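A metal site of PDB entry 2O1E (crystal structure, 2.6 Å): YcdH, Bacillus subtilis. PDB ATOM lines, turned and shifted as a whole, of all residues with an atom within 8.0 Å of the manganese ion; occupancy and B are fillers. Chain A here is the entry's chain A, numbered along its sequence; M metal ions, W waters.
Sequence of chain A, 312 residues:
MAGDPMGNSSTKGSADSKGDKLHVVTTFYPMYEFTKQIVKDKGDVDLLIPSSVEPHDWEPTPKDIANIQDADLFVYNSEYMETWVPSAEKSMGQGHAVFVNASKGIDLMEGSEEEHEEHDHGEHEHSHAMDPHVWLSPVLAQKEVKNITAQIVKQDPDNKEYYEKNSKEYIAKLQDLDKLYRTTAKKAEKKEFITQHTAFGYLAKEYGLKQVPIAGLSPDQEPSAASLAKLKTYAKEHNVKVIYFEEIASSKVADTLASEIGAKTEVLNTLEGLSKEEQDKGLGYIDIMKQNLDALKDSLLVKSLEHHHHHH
The nearest printed residue that does not touch the manganese ion is Ala 199 (4.3 Å).
The manganese ion is bound by a ring nitrogen (NE2) of His 56 (2.1 Å), a ring nitrogen (NE2) of His 133 (2.1 Å), the side-chain carboxylate (OE2) of Glu 272 (2.2 Å) and water W1 (2.5 Å). The manganese ion has four donor atoms within binding distance. Slightly farther from the manganese ion lies OE1 of Glu 272 (2.9 Å).
A ring nitrogen (ND1) of His 56 lies close to the side-chain sulfur (SD) of Met 81, 3.5 Å away. N of His 56 sits at hydrogen-bond distance from OE2 of Glu 54, 2.7 Å away. N of His 133 is in hydrogen-bond range of OD1 of Asp 131, 2.9 Å away. N of Glu 272 lies close to OG1 of Thr 270 (3.4 Å).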
ATOM      1  N   PHE A  28     -14.018  -0.583  35.249  1.00  0.00           N
ATOM      2  CA  PHE A  28     -14.622   0.720  34.978  1.00  0.00           C
ATOM      3  C   PHE A  28     -16.140   0.614  34.732  1.00  0.00           C
ATOM      4  O   PHE A  28     -16.676  -0.483  34.582  1.00  0.00           O
ATOM      5  CB  PHE A  28     -13.912   1.434  33.811  1.00  0.00           C
ATOM      6  CG  PHE A  28     -13.941   0.693  32.501  1.00  0.00           C
ATOM      7  CD1 PHE A  28     -14.213   1.351  31.305  1.00  0.00           C
ATOM      8  CD2 PHE A  28     -13.642  -0.666  32.456  1.00  0.00           C
ATOM      9  CE1 PHE A  28     -14.176   0.673  30.088  1.00  0.00           C
ATOM     10  CE2 PHE A  28     -13.607  -1.354  31.241  1.00  0.00           C
ATOM     11  CZ  PHE A  28     -13.874  -0.685  30.057  1.00  0.00           C
ATOM     12  N   GLU A  54      -9.480   8.269  33.955  1.00  0.00           N
ATOM     13  CA  GLU A  54      -9.041   7.454  32.832  1.00  0.00           C
ATOM     14  C   GLU A  54      -8.776   5.993  33.208  1.00  0.00           C
ATOM     15  O   GLU A  54      -7.836   5.683  33.937  1.00  0.00           O
ATOM     16  CB  GLU A  54      -7.765   8.049  32.229  1.00  0.00           C
ATOM     17  CG  GLU A  54      -6.947   7.072  31.399  1.00  0.00           C
ATOM     18  CD  GLU A  54      -7.638   6.659  30.117  1.00  0.00           C
ATOM     19  OE1 GLU A  54      -7.213   7.127  29.030  1.00  0.00           O
ATOM     20  OE2 GLU A  54      -8.605   5.879  30.190  1.00  0.00           O
ATOM     21  N   PRO A  55      -9.626   5.066  32.706  1.00  0.00           N
ATOM     22  CA  PRO A  55      -9.427   3.644  33.043  1.00  0.00           C
ATOM     23  C   PRO A  55      -8.219   3.023  32.322  1.00  0.00           C
ATOM     24  O   PRO A  55      -7.498   2.196  32.887  1.00  0.00           O
ATOM     25  CB  PRO A  55     -10.756   3.013  32.632  1.00  0.00           C
ATOM     26  CG  PRO A  55     -11.180   3.857  31.482  1.00  0.00           C
ATOM     27  CD  PRO A  55     -10.855   5.255  31.921  1.00  0.00           C
ATOM     28  N   HIS A  56      -8.007   3.430  31.073  1.00  0.00           N
ATOM     29  CA  HIS A  56      -6.910   2.913  30.266  1.00  0.00           C
ATOM     30  C   HIS A  56      -5.584   2.882  31.004  1.00  0.00           C
ATOM     31  O   HIS A  56      -4.859   1.892  30.942  1.00  0.00           O
ATOM     32  CB  HIS A  56      -6.734   3.751  29.002  1.00  0.00           C
ATOM     33  CG  HIS A  56      -7.640   3.350  27.887  1.00  0.00           C
ATOM     34  ND1 HIS A  56      -7.592   2.096  27.307  1.00  0.00           N
ATOM     35  CD2 HIS A  56      -8.645   4.014  27.268  1.00  0.00           C
ATOM     36  CE1 HIS A  56      -8.525   2.012  26.384  1.00  0.00           C
ATOM     37  NE2 HIS A  56      -9.183   3.155  26.333  1.00  0.00           N
ATOM     38  N   MET A  81      -7.446  -3.756  27.672  1.00  0.00           N
ATOM     39  CA  MET A  81      -8.109  -2.621  28.274  1.00  0.00           C
ATOM     40  C   MET A  81      -7.453  -2.406  29.629  1.00  0.00           C
ATOM     41  O   MET A  81      -6.641  -1.502  29.799  1.00  0.00           O
ATOM     42  CB  MET A  81      -9.592  -2.930  28.435  1.00  0.00           C
ATOM     43  CG  MET A  81     -10.391  -1.841  29.147  1.00  0.00           C
ATOM     44  SD  MET A  81     -10.182  -0.098  28.277  1.00  0.00           S
ATOM     45  CE  MET A  81     -11.091  -0.579  26.652  1.00  0.00           C
ATOM     46  N   ASP A 131      -7.958  -3.754  19.798  1.00  0.00           N
ATOM     47  CA  ASP A 131      -8.862  -2.702  20.203  1.00  0.00           C
ATOM     48  C   ASP A 131      -9.870  -3.282  21.207  1.00  0.00           C
ATOM     49  O   ASP A 131     -10.680  -4.135  20.841  1.00  0.00           O
ATOM     50  CB  ASP A 131      -9.605  -2.127  18.997  1.00  0.00           C
ATOM     51  CG  ASP A 131     -10.400  -0.877  19.362  1.00  0.00           C
ATOM     52  OD1 ASP A 131     -11.155  -0.925  20.352  1.00  0.00           O
ATOM     53  OD2 ASP A 131     -10.269   0.141  18.645  1.00  0.00           O
ATOM     54  N   PRO A 132      -9.822  -2.811  22.476  1.00  0.00           N
ATOM     55  CA  PRO A 132     -10.714  -3.283  23.544  1.00  0.00           C
ATOM     56  C   PRO A 132     -12.082  -2.603  23.691  1.00  0.00           C
ATOM     57  O   PRO A 132     -12.873  -2.997  24.543  1.00  0.00           O
ATOM     58  CB  PRO A 132      -9.858  -3.059  24.777  1.00  0.00           C
ATOM     59  CG  PRO A 132      -9.211  -1.750  24.462  1.00  0.00           C
ATOM     60  CD  PRO A 132      -8.808  -1.892  23.021  1.00  0.00           C
ATOM     61  N   HIS A 133     -12.379  -1.613  22.853  1.00  0.00           N
ATOM     62  CA  HIS A 133     -13.648  -0.899  22.965  1.00  0.00           C
ATOM     63  C   HIS A 133     -14.859  -1.628  22.426  1.00  0.00           C
ATOM     64  O   HIS A 133     -15.731  -1.017  21.795  1.00  0.00           O
ATOM     65  CB  HIS A 133     -13.522   0.470  22.300  1.00  0.00           C
ATOM     66  CG  HIS A 133     -12.409   1.297  22.859  1.00  0.00           C
ATOM     67  ND1 HIS A 133     -11.093   1.131  22.481  1.00  0.00           N
ATOM     68  CD2 HIS A 133     -12.408   2.283  23.778  1.00  0.00           C
ATOM     69  CE1 HIS A 133     -10.333   1.980  23.144  1.00  0.00           C
ATOM     70  NE2 HIS A 133     -11.108   2.693  23.934  1.00  0.00           N
ATOM     71  N   TRP A 135     -17.376  -2.933  24.073  1.00  0.00           N
ATOM     72  CA  TRP A 135     -18.616  -2.593  24.737  1.00  0.00           C
ATOM     73  C   TRP A 135     -19.289  -1.423  24.051  1.00  0.00           C
ATOM     74  O   TRP A 135     -20.445  -1.097  24.359  1.00  0.00           O
ATOM     75  CB  TRP A 135     -18.350  -2.261  26.217  1.00  0.00           C
ATOM     76  CG  TRP A 135     -17.848  -0.883  26.396  1.00  0.00           C
ATOM     77  CD1 TRP A 135     -18.590   0.259  26.475  1.00  0.00           C
ATOM     78  CD2 TRP A 135     -16.484  -0.480  26.400  1.00  0.00           C
ATOM     79  NE1 TRP A 135     -17.768   1.355  26.499  1.00  0.00           N
ATOM     80  CE2 TRP A 135     -16.469   0.935  26.451  1.00  0.00           C
ATOM     81  CE3 TRP A 135     -15.275  -1.182  26.345  1.00  0.00           C
ATOM     82  CZ2 TRP A 135     -15.280   1.669  26.468  1.00  0.00           C
ATOM     83  CZ3 TRP A 135     -14.093  -0.447  26.357  1.00  0.00           C
ATOM     84  CH2 TRP A 135     -14.107   0.965  26.415  1.00  0.00           C
ATOM     85  N   LEU A 136     -18.600  -0.759  23.128  1.00  0.00           N
ATOM     86  CA  LEU A 136     -19.238   0.368  22.416  1.00  0.00           C
ATOM     87  C   LEU A 136     -20.055  -0.138  21.218  1.00  0.00           C
ATOM     88  O   LEU A 136     -20.255   0.568  20.234  1.00  0.00           O
ATOM     89  CB  LEU A 136     -18.223   1.419  21.966  1.00  0.00           C
ATOM     90  CG  LEU A 136     -17.680   2.361  23.038  1.00  0.00           C
ATOM     91  CD1 LEU A 136     -16.726   3.359  22.433  1.00  0.00           C
ATOM     92  CD2 LEU A 136     -18.837   3.085  23.699  1.00  0.00           C
ATOM     93  N   HIS A 197     -10.827  11.079  18.074  1.00  0.00           N
ATOM     94  CA  HIS A 197     -10.377   9.863  18.746  1.00  0.00           C
ATOM     95  C   HIS A 197     -10.623   8.642  17.830  1.00  0.00           C
ATOM     96  O   HIS A 197     -10.610   8.785  16.598  1.00  0.00           O
ATOM     97  CB  HIS A 197     -11.142   9.696  20.080  1.00  0.00           C
ATOM     98  CG  HIS A 197     -12.609   9.976  19.992  1.00  0.00           C
ATOM     99  ND1 HIS A 197     -13.458   9.839  21.073  1.00  0.00           N
ATOM    100  CD2 HIS A 197     -13.392  10.391  18.966  1.00  0.00           C
ATOM    101  CE1 HIS A 197     -14.687  10.138  20.715  1.00  0.00           C
ATOM    102  NE2 HIS A 197     -14.680  10.472  19.435  1.00  0.00           N
ATOM    103  N   THR A 198     -10.825   7.462  18.405  1.00  0.00           N
ATOM    104  CA  THR A 198     -11.067   6.283  17.565  1.00  0.00           C
ATOM    105  C   THR A 198     -11.585   5.079  18.328  1.00  0.00           C
ATOM    106  O   THR A 198     -11.471   3.937  17.888  1.00  0.00           O
ATOM    107  CB  THR A 198      -9.797   5.862  16.823  1.00  0.00           C
ATOM    108  OG1 THR A 198     -10.081   4.693  16.050  1.00  0.00           O
ATOM    109  CG2 THR A 198      -8.665   5.587  17.779  1.00  0.00           C
ATOM    110  N   ALA A 199     -12.206   5.346  19.465  1.00  0.00           N
ATOM    111  CA  ALA A 199     -12.728   4.312  20.321  1.00  0.00           C
ATOM    112  C   ALA A 199     -14.019   3.718  19.802  1.00  0.00           C
ATOM    113  O   ALA A 199     -14.561   2.771  20.390  1.00  0.00           O
ATOM    114  CB  ALA A 199     -12.946   4.863  21.718  1.00  0.00           C
ATOM    115  N   PHE A 200     -14.525   4.257  18.703  1.00  0.00           N
ATOM    116  CA  PHE A 200     -15.785   3.776  18.157  1.00  0.00           C
ATOM    117  C   PHE A 200     -15.642   2.793  16.999  1.00  0.00           C
ATOM    118  O   PHE A 200     -16.581   2.588  16.230  1.00  0.00           O
ATOM    119  CB  PHE A 200     -16.663   4.973  17.810  1.00  0.00           C
ATOM    120  CG  PHE A 200     -17.208   5.680  19.021  1.00  0.00           C
ATOM    121  CD1 PHE A 200     -18.442   5.304  19.561  1.00  0.00           C
ATOM    122  CD2 PHE A 200     -16.446   6.635  19.702  1.00  0.00           C
ATOM    123  CE1 PHE A 200     -18.894   5.855  20.766  1.00  0.00           C
ATOM    124  CE2 PHE A 200     -16.897   7.196  20.905  1.00  0.00           C
ATOM    125  CZ  PHE A 200     -18.127   6.808  21.439  1.00  0.00           C
ATOM    126  N   GLU A 246     -14.013  13.226  22.236  1.00  0.00           N
ATOM    127  CA  GLU A 246     -14.184  12.416  23.423  1.00  0.00           C
ATOM    128  C   GLU A 246     -15.022  13.206  24.417  1.00  0.00           C
ATOM    129  O   GLU A 246     -15.999  12.705  24.983  1.00  0.00           O
ATOM    130  CB  GLU A 246     -12.826  12.114  24.006  1.00  0.00           C
ATOM    131  CG  GLU A 246     -12.809  10.955  24.951  1.00  0.00           C
ATOM    132  CD  GLU A 246     -11.602  10.996  25.849  1.00  0.00           C
ATOM    133  OE1 GLU A 246     -10.539  11.449  25.363  1.00  0.00           O
ATOM    134  OE2 GLU A 246     -11.722  10.567  27.027  1.00  0.00           O
ATOM    135  N   THR A 270     -17.346   7.656  24.861  1.00  0.00           N
ATOM    136  CA  THR A 270     -17.076   6.294  25.210  1.00  0.00           C
ATOM    137  C   THR A 270     -17.585   6.164  26.618  1.00  0.00           C
ATOM    138  O   THR A 270     -17.308   7.005  27.471  1.00  0.00           O
ATOM    139  CB  THR A 270     -15.576   6.052  25.198  1.00  0.00           C
ATOM    140  OG1 THR A 270     -14.975   6.678  26.325  1.00  0.00           O
ATOM    141  CG2 THR A 270     -14.975   6.651  23.938  1.00  0.00           C
ATOM    142  N   LEU A 271     -18.361   5.124  26.885  1.00  0.00           N
ATOM    143  CA  LEU A 271     -18.871   4.954  28.231  1.00  0.00           C
ATOM    144  C   LEU A 271     -17.696   4.568  29.138  1.00  0.00           C
ATOM    145  O   LEU A 271     -17.817   3.643  29.930  1.00  0.00           O
ATOM    146  CB  LEU A 271     -19.937   3.857  28.252  1.00  0.00           C
ATOM    147  CG  LEU A 271     -21.416   4.256  28.243  1.00  0.00           C
ATOM    148  CD1 LEU A 271     -21.772   4.878  29.571  1.00  0.00           C
ATOM    149  CD2 LEU A 271     -21.687   5.202  27.097  1.00  0.00           C
ATOM    150  N   GLU A 272     -16.578   5.254  29.017  1.00  0.00           N
ATOM    151  CA  GLU A 272     -15.433   4.926  29.852  1.00  0.00           C
ATOM    152  C   GLU A 272     -15.581   5.526  31.205  1.00  0.00           C
ATOM    153  O   GLU A 272     -14.973   5.080  32.181  1.00  0.00           O
ATOM    154  CB  GLU A 272     -14.139   5.392  29.178  1.00  0.00           C
ATOM    155  CG  GLU A 272     -13.378   4.227  28.585  1.00  0.00           C
ATOM    156  CD  GLU A 272     -12.470   4.603  27.458  1.00  0.00           C
ATOM    157  OE1 GLU A 272     -11.697   5.566  27.624  1.00  0.00           O
ATOM    158  OE2 GLU A 272     -12.515   3.919  26.423  1.00  0.00           O
HETATM  159 MN    MN M   1     -10.642   4.257  25.294  1.00  0.00          MN
HETATM  160  O   HOH W   1      -9.715   6.020  23.855  1.00  0.00           O
